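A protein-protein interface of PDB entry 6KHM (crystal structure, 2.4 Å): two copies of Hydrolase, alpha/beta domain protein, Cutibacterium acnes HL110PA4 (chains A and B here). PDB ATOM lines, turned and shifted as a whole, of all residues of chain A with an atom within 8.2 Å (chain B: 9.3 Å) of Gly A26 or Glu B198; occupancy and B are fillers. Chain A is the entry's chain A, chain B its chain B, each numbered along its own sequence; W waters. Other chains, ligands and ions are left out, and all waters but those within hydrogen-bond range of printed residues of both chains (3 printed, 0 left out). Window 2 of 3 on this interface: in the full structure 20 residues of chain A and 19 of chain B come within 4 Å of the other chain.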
ATOM      1  N   ALA A   2      13.484 -17.921   9.560  1.00  0.00           N
ATOM      2  CA  ALA A   2      13.376 -19.021  10.542  1.00  0.00           C
ATOM      3  C   ALA A   2      14.172 -18.665  11.822  1.00  0.00           C
ATOM      4  O   ALA A   2      15.152 -17.929  11.756  1.00  0.00           O
ATOM      5  CB  ALA A   2      13.847 -20.317   9.915  1.00  0.00           C
ATOM      6  N   GLU A  23      17.787 -17.592  10.597  1.00  0.00           N
ATOM      7  CA  GLU A  23      18.009 -18.050   9.200  1.00  0.00           C
ATOM      8  C   GLU A  23      17.201 -17.159   8.283  1.00  0.00           C
ATOM      9  O   GLU A  23      16.031 -16.919   8.549  1.00  0.00           O
ATOM     10  CB  GLU A  23      17.624 -19.508   9.004  1.00  0.00           C
ATOM     11  CG  GLU A  23      18.429 -20.444   9.890  1.00  0.00           C
ATOM     12  CD  GLU A  23      17.929 -21.873   9.955  1.00  0.00           C
ATOM     13  OE1 GLU A  23      18.032 -22.503  11.035  1.00  0.00           O
ATOM     14  OE2 GLU A  23      17.406 -22.327   8.937  1.00  0.00           O
ATOM     15  N   PRO A  24      17.783 -16.681   7.164  1.00  0.00           N
ATOM     16  CA  PRO A  24      17.022 -15.953   6.167  1.00  0.00           C
ATOM     17  C   PRO A  24      16.207 -16.891   5.279  1.00  0.00           C
ATOM     18  O   PRO A  24      16.401 -18.116   5.257  1.00  0.00           O
ATOM     19  CB  PRO A  24      18.072 -15.235   5.327  1.00  0.00           C
ATOM     20  CG  PRO A  24      19.222 -16.174   5.388  1.00  0.00           C
ATOM     21  CD  PRO A  24      19.177 -16.824   6.760  1.00  0.00           C
ATOM     22  N   VAL A  25      15.283 -16.231   4.599  1.00  0.00           N
ATOM     23  CA  VAL A  25      14.475 -16.735   3.459  1.00  0.00           C
ATOM     24  C   VAL A  25      15.437 -17.011   2.297  1.00  0.00           C
ATOM     25  O   VAL A  25      16.265 -16.128   1.943  1.00  0.00           O
ATOM     26  CB  VAL A  25      13.400 -15.671   3.138  1.00  0.00           C
ATOM     27  CG1 VAL A  25      12.872 -15.801   1.736  1.00  0.00           C
ATOM     28  CG2 VAL A  25      12.273 -15.708   4.168  1.00  0.00           C
ATOM     29  N   GLY A  26      15.377 -18.207   1.736  1.00  0.00           N
ATOM     30  CA  GLY A  26      16.214 -18.551   0.571  1.00  0.00           C
ATOM     31  C   GLY A  26      17.460 -19.305   0.987  1.00  0.00           C
ATOM     32  O   GLY A  26      17.501 -19.814   2.109  1.00  0.00           O
ATOM     33  N   THR A  27      18.422 -19.416   0.079  1.00  0.00           N
ATOM     34  CA  THR A  27      19.704 -20.107   0.321  1.00  0.00           C
ATOM     35  C   THR A  27      20.641 -19.067   0.915  1.00  0.00           C
ATOM     36  O   THR A  27      20.952 -18.059   0.282  1.00  0.00           O
ATOM     37  CB  THR A  27      20.180 -20.805  -0.962  1.00  0.00           C
ATOM     38  OG1 THR A  27      19.028 -21.538  -1.376  1.00  0.00           O
ATOM     39  CG2 THR A  27      21.370 -21.729  -0.764  1.00  0.00           C
ATOM     40  N   PRO A  28      21.078 -19.254   2.179  1.00  0.00           N
ATOM     41  CA  PRO A  28      22.029 -18.325   2.774  1.00  0.00           C
ATOM     42  C   PRO A  28      23.422 -18.529   2.153  1.00  0.00           C
ATOM     43  O   PRO A  28      23.721 -19.654   1.770  1.00  0.00           O
ATOM     44  CB  PRO A  28      21.933 -18.675   4.261  1.00  0.00           C
ATOM     45  CG  PRO A  28      21.599 -20.147   4.264  1.00  0.00           C
ATOM     46  CD  PRO A  28      20.685 -20.354   3.081  1.00  0.00           C
ATOM     47  N   THR A  29      24.237 -17.462   2.095  1.00  0.00           N
ATOM     48  CA  THR A  29      25.570 -17.461   1.436  1.00  0.00           C
ATOM     49  C   THR A  29      26.712 -17.414   2.453  1.00  0.00           C
ATOM     50  O   THR A  29      27.873 -17.619   2.038  1.00  0.00           O
ATOM     51  CB  THR A  29      25.686 -16.298   0.457  1.00  0.00           C
ATOM     52  OG1 THR A  29      25.400 -15.158   1.257  1.00  0.00           O
ATOM     53  CG2 THR A  29      24.764 -16.437  -0.743  1.00  0.00           C
ATOM     54  N   LEU A  53      20.269 -10.658   7.660  1.00  0.00           N
ATOM     55  CA  LEU A  53      19.249 -11.560   7.080  1.00  0.00           C
ATOM     56  C   LEU A  53      18.878 -11.011   5.695  1.00  0.00           C
ATOM     57  O   LEU A  53      18.861 -11.801   4.726  1.00  0.00           O
ATOM     58  CB  LEU A  53      18.051 -11.669   8.028  1.00  0.00           C
ATOM     59  CG  LEU A  53      18.234 -12.497   9.309  1.00  0.00           C
ATOM     60  CD1 LEU A  53      17.131 -12.173  10.326  1.00  0.00           C
ATOM     61  CD2 LEU A  53      18.228 -14.006   9.030  1.00  0.00           C
ATOM     62  N   GLY A  56      21.237 -11.947   3.175  1.00  0.00           N
ATOM     63  CA  GLY A  56      21.154 -13.400   2.883  1.00  0.00           C
ATOM     64  C   GLY A  56      22.125 -14.219   3.717  1.00  0.00           C
ATOM     65  O   GLY A  56      22.688 -15.209   3.179  1.00  0.00           O
ATOM     66  N   VAL A  58      22.935 -16.298   7.496  1.00  0.00           N
ATOM     67  CA  VAL A  58      22.497 -16.876   8.797  1.00  0.00           C
ATOM     68  C   VAL A  58      23.236 -16.054   9.852  1.00  0.00           C
ATOM     69  O   VAL A  58      24.428 -15.778   9.674  1.00  0.00           O
ATOM     70  CB  VAL A  58      22.806 -18.389   8.930  1.00  0.00           C
ATOM     71  CG1 VAL A  58      22.800 -18.854  10.386  1.00  0.00           C
ATOM     72  CG2 VAL A  58      21.863 -19.253   8.089  1.00  0.00           C
ATOM     73  N   PHE A 103      25.360 -25.913   7.990  1.00  0.00           N
ATOM     74  CA  PHE A 103      25.957 -24.871   7.103  1.00  0.00           C
ATOM     75  C   PHE A 103      27.472 -25.075   6.932  1.00  0.00           C
ATOM     76  O   PHE A 103      28.210 -24.063   6.742  1.00  0.00           O
ATOM     77  CB  PHE A 103      25.627 -23.475   7.644  1.00  0.00           C
ATOM     78  CG  PHE A 103      24.144 -23.227   7.788  1.00  0.00           C
ATOM     79  CD1 PHE A 103      23.348 -23.052   6.669  1.00  0.00           C
ATOM     80  CD2 PHE A 103      23.535 -23.261   9.035  1.00  0.00           C
ATOM     81  CE1 PHE A 103      21.980 -22.895   6.798  1.00  0.00           C
ATOM     82  CE2 PHE A 103      22.161 -23.108   9.165  1.00  0.00           C
ATOM     83  CZ  PHE A 103      21.387 -22.939   8.047  1.00  0.00           C
ATOM     84  N   ARG B  44       8.789 -14.001  14.028  1.00  0.00           N
ATOM     85  CA  ARG B  44       8.784 -13.991  12.550  1.00  0.00           C
ATOM     86  C   ARG B  44       8.719 -12.558  12.000  1.00  0.00           C
ATOM     87  O   ARG B  44       9.127 -12.378  10.854  1.00  0.00           O
ATOM     88  CB  ARG B  44       7.577 -14.811  12.083  1.00  0.00           C
ATOM     89  CG  ARG B  44       7.589 -15.183  10.615  1.00  0.00           C
ATOM     90  CD  ARG B  44       6.729 -16.417  10.357  1.00  0.00           C
ATOM     91  NE  ARG B  44       6.816 -16.712   8.942  1.00  0.00           N
ATOM     92  CZ  ARG B  44       5.820 -16.634   8.076  1.00  0.00           C
ATOM     93  NH1 ARG B  44       4.590 -16.351   8.482  1.00  0.00           N
ATOM     94  NH2 ARG B  44       6.042 -16.919   6.799  1.00  0.00           N
ATOM     95  N   ASP B 187       2.859 -25.274  -7.020  1.00  0.00           N
ATOM     96  CA  ASP B 187       2.686 -24.387  -5.852  1.00  0.00           C
ATOM     97  C   ASP B 187       2.743 -25.172  -4.540  1.00  0.00           C
ATOM     98  O   ASP B 187       3.364 -24.692  -3.624  1.00  0.00           O
ATOM     99  CB  ASP B 187       1.350 -23.684  -6.009  1.00  0.00           C
ATOM    100  CG  ASP B 187       1.423 -22.623  -7.073  1.00  0.00           C
ATOM    101  OD1 ASP B 187       2.470 -22.026  -7.196  1.00  0.00           O
ATOM    102  OD2 ASP B 187       0.435 -22.399  -7.729  1.00  0.00           O
ATOM    103  N   VAL B 193       0.114 -19.208   0.752  1.00  0.00           N
ATOM    104  CA  VAL B 193       0.860 -18.403   1.772  1.00  0.00           C
ATOM    105  C   VAL B 193       1.632 -17.251   1.115  1.00  0.00           C
ATOM    106  O   VAL B 193       1.711 -16.157   1.717  1.00  0.00           O
ATOM    107  CB  VAL B 193       1.785 -19.328   2.571  1.00  0.00           C
ATOM    108  CG1 VAL B 193       2.820 -18.563   3.353  1.00  0.00           C
ATOM    109  CG2 VAL B 193       0.990 -20.219   3.510  1.00  0.00           C
ATOM    110  N   ALA B 194       2.204 -17.483  -0.072  1.00  0.00           N
ATOM    111  CA  ALA B 194       2.965 -16.467  -0.833  1.00  0.00           C
ATOM    112  C   ALA B 194       3.263 -16.977  -2.248  1.00  0.00           C
ATOM    113  O   ALA B 194       3.518 -18.213  -2.387  1.00  0.00           O
ATOM    114  CB  ALA B 194       4.230 -16.138  -0.089  1.00  0.00           C
ATOM    115  N   ARG B 195       3.240 -16.054  -3.227  1.00  0.00           N
ATOM    116  CA  ARG B 195       3.789 -16.265  -4.589  1.00  0.00           C
ATOM    117  C   ARG B 195       5.232 -16.766  -4.450  1.00  0.00           C
ATOM    118  O   ARG B 195       5.610 -17.692  -5.209  1.00  0.00           O
ATOM    119  CB  ARG B 195       3.774 -15.005  -5.464  1.00  0.00           C
ATOM    120  CG  ARG B 195       3.272 -15.243  -6.884  1.00  0.00           C
ATOM    121  CD  ARG B 195       3.977 -14.546  -8.032  1.00  0.00           C
ATOM    122  NE  ARG B 195       4.807 -13.396  -7.677  1.00  0.00           N
ATOM    123  CZ  ARG B 195       4.592 -12.114  -8.026  1.00  0.00           C
ATOM    124  NH1 ARG B 195       3.519 -11.744  -8.699  1.00  0.00           N
ATOM    125  NH2 ARG B 195       5.457 -11.178  -7.672  1.00  0.00           N
ATOM    126  N   SER B 196       5.977 -16.200  -3.493  1.00  0.00           N
ATOM    127  CA  SER B 196       7.416 -16.505  -3.229  1.00  0.00           C
ATOM    128  C   SER B 196       7.554 -17.888  -2.594  1.00  0.00           C
ATOM    129  O   SER B 196       7.099 -18.064  -1.438  1.00  0.00           O
ATOM    130  CB  SER B 196       8.083 -15.460  -2.365  1.00  0.00           C
ATOM    131  OG  SER B 196       9.350 -15.931  -1.935  1.00  0.00           O
ATOM    132  N   LYS B 197       8.175 -18.811  -3.328  1.00  0.00           N
ATOM    133  CA  LYS B 197       8.451 -20.216  -2.899  1.00  0.00           C
ATOM    134  C   LYS B 197       9.442 -20.212  -1.725  1.00  0.00           C
ATOM    135  O   LYS B 197       9.326 -21.072  -0.835  1.00  0.00           O
ATOM    136  CB  LYS B 197       8.888 -21.012  -4.138  1.00  0.00           C
ATOM    137  CG  LYS B 197       7.767 -21.161  -5.166  1.00  0.00           C
ATOM    138  CD  LYS B 197       8.201 -21.354  -6.610  1.00  0.00           C
ATOM    139  CE  LYS B 197       8.409 -22.803  -6.990  1.00  0.00           C
ATOM    140  NZ  LYS B 197       7.238 -23.631  -6.626  1.00  0.00           N
ATOM    141  N   GLU B 198      10.345 -19.229  -1.703  1.00  0.00           N
ATOM    142  CA  GLU B 198      11.343 -19.007  -0.623  1.00  0.00           C
ATOM    143  C   GLU B 198      10.590 -18.777   0.713  1.00  0.00           C
ATOM    144  O   GLU B 198      10.950 -19.437   1.707  1.00  0.00           O
ATOM    145  CB  GLU B 198      12.319 -17.884  -1.030  1.00  0.00           C
ATOM    146  CG  GLU B 198      13.160 -18.176  -2.279  1.00  0.00           C
ATOM    147  CD  GLU B 198      14.362 -17.264  -2.552  1.00  0.00           C
ATOM    148  OE1 GLU B 198      14.285 -16.048  -2.287  1.00  0.00           O
ATOM    149  OE2 GLU B 198      15.392 -17.774  -3.043  1.00  0.00           O
ATOM    150  N   VAL B 199       9.526 -17.963   0.728  1.00  0.00           N
ATOM    151  CA  VAL B 199       8.806 -17.592   1.974  1.00  0.00           C
ATOM    152  C   VAL B 199       7.994 -18.816   2.399  1.00  0.00           C
ATOM    153  O   VAL B 199       7.918 -19.073   3.603  1.00  0.00           O
ATOM    154  CB  VAL B 199       7.901 -16.351   1.814  1.00  0.00           C
ATOM    155  CG1 VAL B 199       6.942 -16.186   3.000  1.00  0.00           C
ATOM    156  CG2 VAL B 199       8.693 -15.079   1.610  1.00  0.00           C
ATOM    157  N   VAL B 200       7.408 -19.537   1.445  1.00  0.00           N
ATOM    158  CA  VAL B 200       6.621 -20.779   1.706  1.00  0.00           C
ATOM    159  C   VAL B 200       7.532 -21.854   2.344  1.00  0.00           C
ATOM    160  O   VAL B 200       7.120 -22.456   3.381  1.00  0.00           O
ATOM    161  CB  VAL B 200       5.933 -21.282   0.422  1.00  0.00           C
ATOM    162  CG1 VAL B 200       5.314 -22.662   0.654  1.00  0.00           C
ATOM    163  CG2 VAL B 200       4.896 -20.279  -0.092  1.00  0.00           C
ATOM    164  N   ALA B 201       8.753 -22.057   1.816  1.00  0.00           N
ATOM    165  CA  ALA B 201       9.669 -23.118   2.305  1.00  0.00           C
ATOM    166  C   ALA B 201      10.098 -22.735   3.713  1.00  0.00           C
ATOM    167  O   ALA B 201      10.163 -23.636   4.574  1.00  0.00           O
ATOM    168  CB  ALA B 201      10.860 -23.325   1.391  1.00  0.00           C
ATOM    169  N   ASP B 202      10.367 -21.444   3.925  1.00  0.00           N
ATOM    170  CA  ASP B 202      10.806 -20.906   5.234  1.00  0.00           C
ATOM    171  C   ASP B 202       9.655 -21.059   6.221  1.00  0.00           C
ATOM    172  O   ASP B 202       9.912 -21.466   7.310  1.00  0.00           O
ATOM    173  CB  ASP B 202      11.245 -19.446   5.149  1.00  0.00           C
ATOM    174  CG  ASP B 202      11.575 -18.901   6.528  1.00  0.00           C
ATOM    175  OD1 ASP B 202      12.636 -19.247   7.065  1.00  0.00           O
ATOM    176  OD2 ASP B 202      10.759 -18.150   7.066  1.00  0.00           O
ATOM    177  N   HIS B 203       8.430 -20.736   5.815  1.00  0.00           N
ATOM    178  CA  HIS B 203       7.206 -20.964   6.612  1.00  0.00           C
ATOM    179  C   HIS B 203       7.155 -22.420   7.080  1.00  0.00           C
ATOM    180  O   HIS B 203       6.750 -22.637   8.218  1.00  0.00           O
ATOM    181  CB  HIS B 203       5.967 -20.653   5.784  1.00  0.00           C
ATOM    182  CG  HIS B 203       4.702 -20.782   6.566  1.00  0.00           C
ATOM    183  ND1 HIS B 203       3.882 -21.892   6.460  1.00  0.00           N
ATOM    184  CD2 HIS B 203       4.083 -19.919   7.406  1.00  0.00           C
ATOM    185  CE1 HIS B 203       2.821 -21.723   7.229  1.00  0.00           C
ATOM    186  NE2 HIS B 203       2.911 -20.509   7.825  1.00  0.00           N
ATOM    187  N   GLY B 204       7.502 -23.373   6.201  1.00  0.00           N
ATOM    188  CA  GLY B 204       7.472 -24.816   6.499  1.00  0.00           C
ATOM    189  C   GLY B 204       8.584 -25.231   7.468  1.00  0.00           C
ATOM    190  O   GLY B 204       8.328 -26.099   8.299  1.00  0.00           O
ATOM    191  N   LYS B 205       9.767 -24.612   7.393  1.00  0.00           N
ATOM    192  CA  LYS B 205      10.993 -25.052   8.127  1.00  0.00           C
ATOM    193  C   LYS B 205      10.996 -24.457   9.554  1.00  0.00           C
ATOM    194  O   LYS B 205      11.422 -25.139  10.489  1.00  0.00           O
ATOM    195  CB  LYS B 205      12.230 -24.702   7.282  1.00  0.00           C
ATOM    196  CG  LYS B 205      13.555 -24.654   8.031  1.00  0.00           C
ATOM    197  CD  LYS B 205      14.764 -25.006   7.183  1.00  0.00           C
ATOM    198  CE  LYS B 205      15.101 -23.964   6.136  1.00  0.00           C
ATOM    199  NZ  LYS B 205      15.874 -22.847   6.732  1.00  0.00           N
ATOM    200  N   ASP B 206      10.517 -23.223   9.726  1.00  0.00           N
ATOM    201  CA  ASP B 206      10.553 -22.471  11.009  1.00  0.00           C
ATOM    202  C   ASP B 206      10.002 -23.378  12.115  1.00  0.00           C
ATOM    203  O   ASP B 206       8.788 -23.657  12.136  1.00  0.00           O
ATOM    204  CB  ASP B 206       9.800 -21.142  10.897  1.00  0.00           C
ATOM    205  CG  ASP B 206      10.214 -20.125  11.954  1.00  0.00           C
ATOM    206  OD1 ASP B 206      10.854 -20.542  12.956  1.00  0.00           O
ATOM    207  OD2 ASP B 206       9.938 -18.915  11.739  1.00  0.00           O
ATOM    208  N   GLU B 286       0.652 -13.515   2.609  1.00  0.00           N
ATOM    209  CA  GLU B 286       1.681 -12.851   3.454  1.00  0.00           C
ATOM    210  C   GLU B 286       2.351 -11.704   2.676  1.00  0.00           C
ATOM    211  O   GLU B 286       3.553 -11.766   2.450  1.00  0.00           O
ATOM    212  CB  GLU B 286       2.681 -13.904   3.944  1.00  0.00           C
ATOM    213  CG  GLU B 286       2.073 -14.942   4.891  1.00  0.00           C
ATOM    214  CD  GLU B 286       3.056 -15.781   5.686  1.00  0.00           C
ATOM    215  OE1 GLU B 286       4.246 -15.793   5.342  1.00  0.00           O
ATOM    216  OE2 GLU B 286       2.635 -16.414   6.667  1.00  0.00           O
ATOM    217  N   ASN B 289       5.415 -10.300   3.870  1.00  0.00           N
ATOM    218  CA  ASN B 289       6.667 -11.102   3.760  1.00  0.00           C
ATOM    219  C   ASN B 289       7.078 -11.238   2.293  1.00  0.00           C
ATOM    220  O   ASN B 289       8.261 -11.556   2.093  1.00  0.00           O
ATOM    221  CB  ASN B 289       6.568 -12.471   4.436  1.00  0.00           C
ATOM    222  CG  ASN B 289       6.422 -12.374   5.935  1.00  0.00           C
ATOM    223  OD1 ASN B 289       7.023 -11.500   6.581  1.00  0.00           O
ATOM    224  ND2 ASN B 289       5.615 -13.276   6.488  1.00  0.00           N
ATOM    225  N   GLU B 290       6.176 -10.994   1.329  1.00  0.00           N
ATOM    226  CA  GLU B 290       6.498 -11.117  -0.114  1.00  0.00           C
ATOM    227  C   GLU B 290       7.519 -10.042  -0.457  1.00  0.00           C
ATOM    228  O   GLU B 290       7.262  -8.861  -0.209  1.00  0.00           O
ATOM    229  CB  GLU B 290       5.280 -10.922  -1.018  1.00  0.00           C
ATOM    230  CG  GLU B 290       4.182 -11.928  -0.795  1.00  0.00           C
ATOM    231  CD  GLU B 290       4.100 -13.048  -1.810  1.00  0.00           C
ATOM    232  OE1 GLU B 290       5.140 -13.540  -2.236  1.00  0.00           O
ATOM    233  OE2 GLU B 290       2.984 -13.426  -2.143  1.00  0.00           O
ATOM    234  N   PRO B 291       8.667 -10.409  -1.072  1.00  0.00           N
ATOM    235  CA  PRO B 291       9.735  -9.446  -1.343  1.00  0.00           C
ATOM    236  C   PRO B 291       9.365  -8.284  -2.288  1.00  0.00           C
ATOM    237  O   PRO B 291       9.958  -7.267  -2.161  1.00  0.00           O
ATOM    238  CB  PRO B 291      10.892 -10.282  -1.911  1.00  0.00           C
ATOM    239  CG  PRO B 291      10.234 -11.567  -2.388  1.00  0.00           C
ATOM    240  CD  PRO B 291       8.982 -11.759  -1.546  1.00  0.00           C
ATOM    241  N   GLU B 292       8.353  -8.384  -3.146  1.00  0.00           N
ATOM    242  CA  GLU B 292       7.997  -7.195  -3.982  1.00  0.00           C
ATOM    243  C   GLU B 292       7.088  -6.243  -3.188  1.00  0.00           C
ATOM    244  O   GLU B 292       7.151  -5.017  -3.500  1.00  0.00           O
ATOM    245  CB  GLU B 292       7.498  -7.504  -5.405  1.00  0.00           C
ATOM    246  CG  GLU B 292       6.726  -8.791  -5.570  1.00  0.00           C
ATOM    247  CD  GLU B 292       7.524 -10.089  -5.544  1.00  0.00           C
ATOM    248  OE1 GLU B 292       8.566 -10.162  -6.228  1.00  0.00           O
ATOM    249  OE2 GLU B 292       7.076 -11.043  -4.846  1.00  0.00           O
HETATM  250  O   HOH W   1      13.593 -20.526   1.858  1.00  0.00           O
HETATM  251  O   HOH W   2      11.787 -16.375  11.349  1.00  0.00           O
HETATM  252  O   HOH W   3      14.649 -20.411   6.035  1.00  0.00           O
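Printed residues of chain B within 4 Å of Val A25: Glu B198 and Asp B202.
Gly A26 touches just one residue of chain B: Glu B198.
Of the printed residues of chain A, Glu B198 touches Val A25 and Gly A26.
Printed residues of chain A within 4 Å of Asp B206: Ala A2 (3.6 Å).
The nearest printed residue of chain A that does not touch Lys B205 is Ala A2 (4.5 Å).
Printed residues of chain B that touch a printed residue of chain A: Glu B198, Asp B202, Lys B205 and Asp B206.
Hydrophobic or aromatic side chains of chain A that line the printed part of chain B: Ala A2 and Val A25.
Among the printed residues, 6 pairs touch across the chains.
Water W3 lies within hydrogen-bond range of OD1 of Asp B202 (2.5 Å), NZ of Lys B205 (2.8 Å) and O of Pro A24 (3.0 Å).
Water W1 bridges the backbone carbonyl oxygen (O) of Glu B198 (2.9 Å) and the backbone NH (N) of Gly A26 (2.9 Å).
Water W2 bridges the backbone NH (N) of Ala A2 (2.9 Å) and the side-chain carboxylate (OD2) of Asp B206 (3.2 Å).
Among the printed residues, pairs that only touch across the chains: Ala A2 with Asp B206 (3.6 Å), Val A25 with Glu B198 (3.5 Å), Val A25 with Asp B202 (3.999 Å) and Gly A26 with Glu B198 (3.8 Å).
N of Ala A2 lies within hydrogen-bond range of OD1 of Asp B202 (2.9 Å).
The side-chain amino group (NZ) of Lys B205 lies within salt-bridge range of the side-chain carboxylate (OE2) of Glu A23 (2.7 Å).
The backbone NH of Glu A23 is in hydrogen-bond range of the backbone carbonyl oxygen of Ala A2 (2.9 Å).
N of Glu B198 sits close to OG of Ser B196 (3.5 Å).
No position is printed for both chains.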
